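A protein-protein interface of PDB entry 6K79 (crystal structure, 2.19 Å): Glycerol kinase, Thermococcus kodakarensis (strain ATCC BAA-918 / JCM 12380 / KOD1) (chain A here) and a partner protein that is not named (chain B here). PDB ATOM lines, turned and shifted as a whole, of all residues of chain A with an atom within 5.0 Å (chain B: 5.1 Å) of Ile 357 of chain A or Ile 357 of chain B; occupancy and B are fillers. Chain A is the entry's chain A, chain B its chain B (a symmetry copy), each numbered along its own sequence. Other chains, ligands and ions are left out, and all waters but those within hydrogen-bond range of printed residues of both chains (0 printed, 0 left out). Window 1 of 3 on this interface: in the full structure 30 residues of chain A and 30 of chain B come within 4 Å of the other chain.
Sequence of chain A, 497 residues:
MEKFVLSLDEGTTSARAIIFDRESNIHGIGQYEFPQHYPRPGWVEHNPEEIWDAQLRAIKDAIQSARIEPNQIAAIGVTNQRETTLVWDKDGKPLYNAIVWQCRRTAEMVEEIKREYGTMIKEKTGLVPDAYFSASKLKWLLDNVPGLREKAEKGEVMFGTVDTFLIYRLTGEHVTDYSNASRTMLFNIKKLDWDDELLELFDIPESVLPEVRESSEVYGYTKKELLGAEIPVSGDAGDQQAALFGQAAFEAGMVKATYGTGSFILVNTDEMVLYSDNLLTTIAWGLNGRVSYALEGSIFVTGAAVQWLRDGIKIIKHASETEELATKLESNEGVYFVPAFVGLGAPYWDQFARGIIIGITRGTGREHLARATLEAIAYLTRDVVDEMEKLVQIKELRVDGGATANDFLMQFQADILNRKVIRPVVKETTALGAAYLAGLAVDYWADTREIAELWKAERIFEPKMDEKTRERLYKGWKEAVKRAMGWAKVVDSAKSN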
ATOM      1  N   TRP A 308       8.443  20.223 -24.645  1.00  0.00           N
ATOM      2  CA  TRP A 308       9.809  20.050 -25.138  1.00  0.00           C
ATOM      3  C   TRP A 308      10.807  20.450 -24.046  1.00  0.00           C
ATOM      4  O   TRP A 308      11.769  19.750 -23.817  1.00  0.00           O
ATOM      5  CB  TRP A 308      10.072  20.848 -26.420  1.00  0.00           C
ATOM      6  CG  TRP A 308      11.503  20.759 -26.843  1.00  0.00           C
ATOM      7  CD1 TRP A 308      12.127  19.662 -27.362  1.00  0.00           C
ATOM      8  CD2 TRP A 308      12.503  21.785 -26.763  1.00  0.00           C
ATOM      9  NE1 TRP A 308      13.444  19.937 -27.618  1.00  0.00           N
ATOM     10  CE2 TRP A 308      13.707  21.228 -27.249  1.00  0.00           C
ATOM     11  CE3 TRP A 308      12.514  23.102 -26.310  1.00  0.00           C
ATOM     12  CZ2 TRP A 308      14.903  21.946 -27.294  1.00  0.00           C
ATOM     13  CZ3 TRP A 308      13.686  23.821 -26.386  1.00  0.00           C
ATOM     14  CH2 TRP A 308      14.870  23.244 -26.849  1.00  0.00           C
ATOM     15  N   VAL A 335      16.155  37.375 -25.314  1.00  0.00           N
ATOM     16  CA  VAL A 335      16.078  35.982 -25.673  1.00  0.00           C
ATOM     17  C   VAL A 335      14.665  35.641 -26.164  1.00  0.00           C
ATOM     18  O   VAL A 335      13.654  35.833 -25.422  1.00  0.00           O
ATOM     19  CB  VAL A 335      16.478  35.138 -24.463  1.00  0.00           C
ATOM     20  CG1 VAL A 335      16.499  33.667 -24.814  1.00  0.00           C
ATOM     21  CG2 VAL A 335      17.823  35.607 -23.922  1.00  0.00           C
ATOM     22  N   TYR A 336      14.621  35.125 -27.387  1.00  0.00           N
ATOM     23  CA  TYR A 336      13.383  34.704 -28.059  1.00  0.00           C
ATOM     24  C   TYR A 336      13.487  33.220 -28.434  1.00  0.00           C
ATOM     25  O   TYR A 336      14.568  32.696 -28.733  1.00  0.00           O
ATOM     26  CB  TYR A 336      13.111  35.605 -29.262  1.00  0.00           C
ATOM     27  CG  TYR A 336      12.553  36.966 -28.910  1.00  0.00           C
ATOM     28  CD1 TYR A 336      13.365  37.984 -28.433  1.00  0.00           C
ATOM     29  CD2 TYR A 336      11.197  37.233 -29.027  1.00  0.00           C
ATOM     30  CE1 TYR A 336      12.856  39.222 -28.068  1.00  0.00           C
ATOM     31  CE2 TYR A 336      10.665  38.456 -28.647  1.00  0.00           C
ATOM     32  CZ  TYR A 336      11.494  39.449 -28.166  1.00  0.00           C
ATOM     33  OH  TYR A 336      10.973  40.665 -27.885  1.00  0.00           O
ATOM     34  N   PHE A 337      12.353  32.544 -28.452  1.00  0.00           N
ATOM     35  CA  PHE A 337      12.268  31.143 -28.857  1.00  0.00           C
ATOM     36  C   PHE A 337      11.076  31.056 -29.781  1.00  0.00           C
ATOM     37  O   PHE A 337       9.944  31.338 -29.342  1.00  0.00           O
ATOM     38  CB  PHE A 337      12.078  30.227 -27.639  1.00  0.00           C
ATOM     39  CG  PHE A 337      11.857  28.752 -27.884  1.00  0.00           C
ATOM     40  CD1 PHE A 337      12.236  28.132 -29.057  1.00  0.00           C
ATOM     41  CD2 PHE A 337      11.318  27.957 -26.892  1.00  0.00           C
ATOM     42  CE1 PHE A 337      12.064  26.769 -29.237  1.00  0.00           C
ATOM     43  CE2 PHE A 337      11.127  26.596 -27.070  1.00  0.00           C
ATOM     44  CZ  PHE A 337      11.514  26.004 -28.241  1.00  0.00           C
ATOM     45  N   GLY A 355      12.603  25.417 -35.347  1.00  0.00           N
ATOM     46  CA  GLY A 355      12.796  26.119 -34.042  1.00  0.00           C
ATOM     47  C   GLY A 355      14.141  26.810 -33.928  1.00  0.00           C
ATOM     48  O   GLY A 355      15.168  26.283 -34.391  1.00  0.00           O
ATOM     49  N   ILE A 356      14.078  28.011 -33.355  1.00  0.00           N
ATOM     50  CA  ILE A 356      15.206  28.924 -33.102  1.00  0.00           C
ATOM     51  C   ILE A 356      15.094  29.415 -31.658  1.00  0.00           C
ATOM     52  O   ILE A 356      14.013  29.859 -31.195  1.00  0.00           O
ATOM     53  CB  ILE A 356      15.200  30.140 -34.066  1.00  0.00           C
ATOM     54  CG1 ILE A 356      15.181  29.697 -35.521  1.00  0.00           C
ATOM     55  CG2 ILE A 356      16.382  31.072 -33.848  1.00  0.00           C
ATOM     56  CD1 ILE A 356      16.168  30.460 -36.397  1.00  0.00           C
ATOM     57  N   ILE A 357      16.204  29.360 -30.968  1.00  0.00           N
ATOM     58  CA  ILE A 357      16.401  30.177 -29.774  1.00  0.00           C
ATOM     59  C   ILE A 357      17.489  31.186 -30.111  1.00  0.00           C
ATOM     60  O   ILE A 357      18.592  30.787 -30.563  1.00  0.00           O
ATOM     61  CB  ILE A 357      16.824  29.343 -28.554  1.00  0.00           C
ATOM     62  CG1 ILE A 357      15.790  28.281 -28.161  1.00  0.00           C
ATOM     63  CG2 ILE A 357      17.119  30.270 -27.411  1.00  0.00           C
ATOM     64  CD1 ILE A 357      16.381  27.093 -27.405  1.00  0.00           C
ATOM     65  N   ILE A 358      17.215  32.466 -29.845  1.00  0.00           N
ATOM     66  CA  ILE A 358      18.164  33.504 -30.193  1.00  0.00           C
ATOM     67  C   ILE A 358      18.242  34.558 -29.089  1.00  0.00           C
ATOM     68  O   ILE A 358      17.273  34.814 -28.336  1.00  0.00           O
ATOM     69  CB  ILE A 358      17.821  34.081 -31.581  1.00  0.00           C
ATOM     70  CG1 ILE A 358      18.913  35.025 -32.079  1.00  0.00           C
ATOM     71  CG2 ILE A 358      16.444  34.733 -31.607  1.00  0.00           C
ATOM     72  CD1 ILE A 358      18.764  35.421 -33.516  1.00  0.00           C
ATOM     73  N   GLY A 359      19.441  35.157 -28.995  1.00  0.00           N
ATOM     74  CA  GLY A 359      19.779  36.140 -27.959  1.00  0.00           C
ATOM     75  C   GLY A 359      20.616  35.534 -26.851  1.00  0.00           C
ATOM     76  O   GLY A 359      20.693  36.071 -25.768  1.00  0.00           O
ATOM     77  N   ILE A 360      21.251  34.400 -27.125  1.00  0.00           N
ATOM     78  CA  ILE A 360      21.985  33.684 -26.088  1.00  0.00           C
ATOM     79  C   ILE A 360      23.339  34.348 -25.790  1.00  0.00           C
ATOM     80  O   ILE A 360      24.127  34.660 -26.692  1.00  0.00           O
ATOM     81  CB  ILE A 360      22.163  32.204 -26.468  1.00  0.00           C
ATOM     82  CG1 ILE A 360      20.828  31.524 -26.736  1.00  0.00           C
ATOM     83  CG2 ILE A 360      22.984  31.479 -25.416  1.00  0.00           C
ATOM     84  CD1 ILE A 360      20.970  30.268 -27.537  1.00  0.00           C
ATOM     85  N   LEU A 369      14.891  30.605 -21.036  1.00  0.00           N
ATOM     86  CA  LEU A 369      14.264  29.639 -21.909  1.00  0.00           C
ATOM     87  C   LEU A 369      12.780  29.464 -21.521  1.00  0.00           C
ATOM     88  O   LEU A 369      11.937  29.404 -22.383  1.00  0.00           O
ATOM     89  CB  LEU A 369      15.026  28.317 -21.838  1.00  0.00           C
ATOM     90  CG  LEU A 369      15.913  28.010 -23.049  1.00  0.00           C
ATOM     91  CD1 LEU A 369      16.860  29.164 -23.360  1.00  0.00           C
ATOM     92  CD2 LEU A 369      16.714  26.724 -22.847  1.00  0.00           C
ATOM     93  N   TRP B 308      28.635  26.978 -20.770  1.00  0.00           N
ATOM     94  CA  TRP B 308      27.240  27.420 -20.800  1.00  0.00           C
ATOM     95  C   TRP B 308      26.262  26.238 -20.765  1.00  0.00           C
ATOM     96  O   TRP B 308      25.223  26.305 -20.073  1.00  0.00           O
ATOM     97  CB  TRP B 308      26.996  28.320 -22.008  1.00  0.00           C
ATOM     98  CG  TRP B 308      25.568  28.745 -22.115  1.00  0.00           C
ATOM     99  CD1 TRP B 308      24.928  29.671 -21.343  1.00  0.00           C
ATOM    100  CD2 TRP B 308      24.572  28.182 -22.993  1.00  0.00           C
ATOM    101  NE1 TRP B 308      23.611  29.740 -21.700  1.00  0.00           N
ATOM    102  CE2 TRP B 308      23.367  28.868 -22.726  1.00  0.00           C
ATOM    103  CE3 TRP B 308      24.593  27.187 -23.981  1.00  0.00           C
ATOM    104  CZ2 TRP B 308      22.181  28.572 -23.392  1.00  0.00           C
ATOM    105  CZ3 TRP B 308      23.428  26.906 -24.657  1.00  0.00           C
ATOM    106  CH2 TRP B 308      22.231  27.580 -24.355  1.00  0.00           C
ATOM    107  N   VAL B 335      20.615  20.455 -36.498  1.00  0.00           N
ATOM    108  CA  VAL B 335      20.719  21.360 -35.346  1.00  0.00           C
ATOM    109  C   VAL B 335      22.121  21.985 -35.254  1.00  0.00           C
ATOM    110  O   VAL B 335      23.111  21.295 -35.227  1.00  0.00           O
ATOM    111  CB  VAL B 335      20.339  20.633 -34.049  1.00  0.00           C
ATOM    112  CG1 VAL B 335      20.491  21.526 -32.831  1.00  0.00           C
ATOM    113  CG2 VAL B 335      18.929  20.096 -34.120  1.00  0.00           C
ATOM    114  N   TYR B 336      22.173  23.310 -35.255  1.00  0.00           N
ATOM    115  CA  TYR B 336      23.390  24.068 -35.121  1.00  0.00           C
ATOM    116  C   TYR B 336      23.265  25.051 -33.963  1.00  0.00           C
ATOM    117  O   TYR B 336      22.180  25.416 -33.570  1.00  0.00           O
ATOM    118  CB  TYR B 336      23.693  24.855 -36.397  1.00  0.00           C
ATOM    119  CG  TYR B 336      24.184  24.031 -37.559  1.00  0.00           C
ATOM    120  CD1 TYR B 336      23.351  23.133 -38.210  1.00  0.00           C
ATOM    121  CD2 TYR B 336      25.485  24.135 -38.005  1.00  0.00           C
ATOM    122  CE1 TYR B 336      23.782  22.375 -39.291  1.00  0.00           C
ATOM    123  CE2 TYR B 336      25.943  23.373 -39.073  1.00  0.00           C
ATOM    124  CZ  TYR B 336      25.089  22.502 -39.729  1.00  0.00           C
ATOM    125  OH  TYR B 336      25.544  21.788 -40.807  1.00  0.00           O
ATOM    126  N   PHE B 337      24.406  25.478 -33.481  1.00  0.00           N
ATOM    127  CA  PHE B 337      24.521  26.431 -32.420  1.00  0.00           C
ATOM    128  C   PHE B 337      25.720  27.323 -32.731  1.00  0.00           C
ATOM    129  O   PHE B 337      26.847  26.827 -32.818  1.00  0.00           O
ATOM    130  CB  PHE B 337      24.695  25.678 -31.093  1.00  0.00           C
ATOM    131  CG  PHE B 337      24.949  26.477 -29.841  1.00  0.00           C
ATOM    132  CD1 PHE B 337      24.529  27.791 -29.700  1.00  0.00           C
ATOM    133  CD2 PHE B 337      25.555  25.868 -28.753  1.00  0.00           C
ATOM    134  CE1 PHE B 337      24.741  28.481 -28.516  1.00  0.00           C
ATOM    135  CE2 PHE B 337      25.761  26.553 -27.562  1.00  0.00           C
ATOM    136  CZ  PHE B 337      25.355  27.862 -27.447  1.00  0.00           C
ATOM    137  N   GLY B 355      24.086  34.641 -29.628  1.00  0.00           N
ATOM    138  CA  GLY B 355      23.984  33.209 -29.755  1.00  0.00           C
ATOM    139  C   GLY B 355      22.647  32.786 -30.336  1.00  0.00           C
ATOM    140  O   GLY B 355      21.580  33.413 -30.079  1.00  0.00           O
ATOM    141  N   ILE B 356      22.691  31.717 -31.113  1.00  0.00           N
ATOM    142  CA  ILE B 356      21.501  31.168 -31.737  1.00  0.00           C
ATOM    143  C   ILE B 356      21.594  29.640 -31.767  1.00  0.00           C
ATOM    144  O   ILE B 356      22.651  29.059 -32.070  1.00  0.00           O
ATOM    145  CB  ILE B 356      21.277  31.748 -33.152  1.00  0.00           C
ATOM    146  CG1 ILE B 356      20.106  31.072 -33.868  1.00  0.00           C
ATOM    147  CG2 ILE B 356      22.535  31.680 -33.998  1.00  0.00           C
ATOM    148  CD1 ILE B 356      19.916  31.560 -35.294  1.00  0.00           C
ATOM    149  N   ILE B 357      20.496  28.990 -31.392  1.00  0.00           N
ATOM    150  CA  ILE B 357      20.358  27.556 -31.660  1.00  0.00           C
ATOM    151  C   ILE B 357      19.235  27.421 -32.678  1.00  0.00           C
ATOM    152  O   ILE B 357      18.163  28.015 -32.450  1.00  0.00           O
ATOM    153  CB  ILE B 357      20.054  26.772 -30.376  1.00  0.00           C
ATOM    154  CG1 ILE B 357      21.162  26.951 -29.339  1.00  0.00           C
ATOM    155  CG2 ILE B 357      19.774  25.308 -30.697  1.00  0.00           C
ATOM    156  CD1 ILE B 357      20.830  26.405 -27.981  1.00  0.00           C
ATOM    157  N   ILE B 358      19.466  26.667 -33.757  1.00  0.00           N
ATOM    158  CA  ILE B 358      18.510  26.568 -34.820  1.00  0.00           C
ATOM    159  C   ILE B 358      18.366  25.111 -35.292  1.00  0.00           C
ATOM    160  O   ILE B 358      19.282  24.280 -35.178  1.00  0.00           O
ATOM    161  CB  ILE B 358      18.910  27.502 -35.973  1.00  0.00           C
ATOM    162  CG1 ILE B 358      17.771  27.641 -36.981  1.00  0.00           C
ATOM    163  CG2 ILE B 358      20.212  27.055 -36.640  1.00  0.00           C
ATOM    164  CD1 ILE B 358      18.036  28.674 -38.014  1.00  0.00           C
ATOM    165  N   GLY B 359      17.188  24.825 -35.848  1.00  0.00           N
ATOM    166  CA  GLY B 359      16.852  23.469 -36.290  1.00  0.00           C
ATOM    167  C   GLY B 359      16.116  22.689 -35.216  1.00  0.00           C
ATOM    168  O   GLY B 359      16.071  21.471 -35.275  1.00  0.00           O
ATOM    169  N   ILE B 360      15.551  23.368 -34.215  1.00  0.00           N
ATOM    170  CA  ILE B 360      14.885  22.651 -33.094  1.00  0.00           C
ATOM    171  C   ILE B 360      13.548  22.060 -33.575  1.00  0.00           C
ATOM    172  O   ILE B 360      12.764  22.736 -34.253  1.00  0.00           O
ATOM    173  CB  ILE B 360      14.691  23.551 -31.857  1.00  0.00           C
ATOM    174  CG1 ILE B 360      15.999  24.164 -31.364  1.00  0.00           C
ATOM    175  CG2 ILE B 360      14.015  22.788 -30.743  1.00  0.00           C
ATOM    176  CD1 ILE B 360      15.812  25.385 -30.488  1.00  0.00           C
ATOM    177  N   LEU B 369      22.063  19.280 -28.673  1.00  0.00           N
ATOM    178  CA  LEU B 369      22.714  20.498 -28.166  1.00  0.00           C
ATOM    179  C   LEU B 369      24.208  20.224 -27.898  1.00  0.00           C
ATOM    180  O   LEU B 369      25.024  21.086 -28.154  1.00  0.00           O
ATOM    181  CB  LEU B 369      22.024  20.976 -26.881  1.00  0.00           C
ATOM    182  CG  LEU B 369      20.945  22.031 -27.073  1.00  0.00           C
ATOM    183  CD1 LEU B 369      20.025  21.659 -28.217  1.00  0.00           C
ATOM    184  CD2 LEU B 369      20.145  22.247 -25.798  1.00  0.00           C
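Of chain A, only Gly 355, Ile 356, Ile 357 and Ile 360 come within 4 Å of Ile 357 of chain B. Of the printed residues of chain B, Ile 360 of chain A touches Trp 308, Gly 355 and Ile 357. Printed residues of chain A within 4 Å of Gly 355 of chain B: Ile 358, Gly 359 and Ile 360. Printed residues of chain A within 4 Å of Ile 356 of chain B: Ile 356 and Ile 357. Of the printed residues of chain B, Ile 356 of chain A touches Ile 356 (3.7 Å), Ile 357 (3.2 Å) and Ile 358 (3.0 Å). Printed residues of chain B within 4 Å of Gly 355 of chain A: Ile 357, Ile 358, Gly 359 and Ile 360. Phe 337 of chain A touches none of the printed residues of chain B. Val 335 of chain A touches none of the printed residues of chain B. The nearest printed residue of chain B that does not touch Ile 357 of chain A is Gly 355 of chain B (4.01 Å).
Among the printed residues, pairs that only touch across the chains: Ile 356 of chain A with Ile 358 of chain B, Ile 357 of chain A with Ile 356 of chain B, Ile 356 of chain A with Ile 357 of chain B, Gly 355 of chain A with Ile 358 of chain B, Ile 358 of chain A with Gly 355 of chain B, Ile 357 of chain A with Ile 360 of chain B, Ile 360 of chain A with Trp 308 of chain B, Trp 308 of chain A with Ile 360 of chain B, Ile 356 of chain A with Ile 356 of chain B, Ile 360 of chain A with Ile 357 of chain B and Gly 355 of chain A with Ile 357 of chain B.
The backbone carbonyl oxygen (O) of Ile 360 of chain B lies within hydrogen-bond range of the backbone NH (N) of Gly 355 of chain A (2.9 Å). The backbone carbonyl oxygen (O) of Ile 357 of chain A lies within hydrogen-bond range of the backbone NH (N) of Ile 357 of chain B, 2.7 Å away. The backbone carbonyl oxygen (O) of Gly 355 of chain B lies within hydrogen-bond range of the backbone NH (N) of Gly 359 of chain A (3.0 Å). The backbone NH (N) of Gly 355 of chain B is in hydrogen-bond range of the backbone carbonyl oxygen (O) of Ile 360 of chain A (2.9 Å). The backbone NH of Gly 359 of chain B is in hydrogen-bond range of the backbone carbonyl oxygen of Gly 355 of chain A (2.9 Å).
Hydrophobic or aromatic side chains of chain A within 4 Å of the printed part of chain B: Trp 308, Ile 356, Ile 357, Ile 358 and Ile 360. Along chain A the printed residues that touch a printed residue of chain B span positions 308 to 360. Of the 11 printed residues of chain B, 7 touch a printed residue of chain A. Hydrophobic or aromatic side chains of chain B within 4 Å of the printed part of chain A: Trp 308, Ile 356, Ile 357, Ile 358 and Ile 360.
The backbone NH (N) of Tyr 336 of chain A is in hydrogen-bond range of the backbone carbonyl oxygen (O) of Ile 358 of chain A, at 2.8 Å. N of Ile 358 of chain B sits at hydrogen-bond distance from O of Tyr 336 of chain B, 3.0 Å away.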
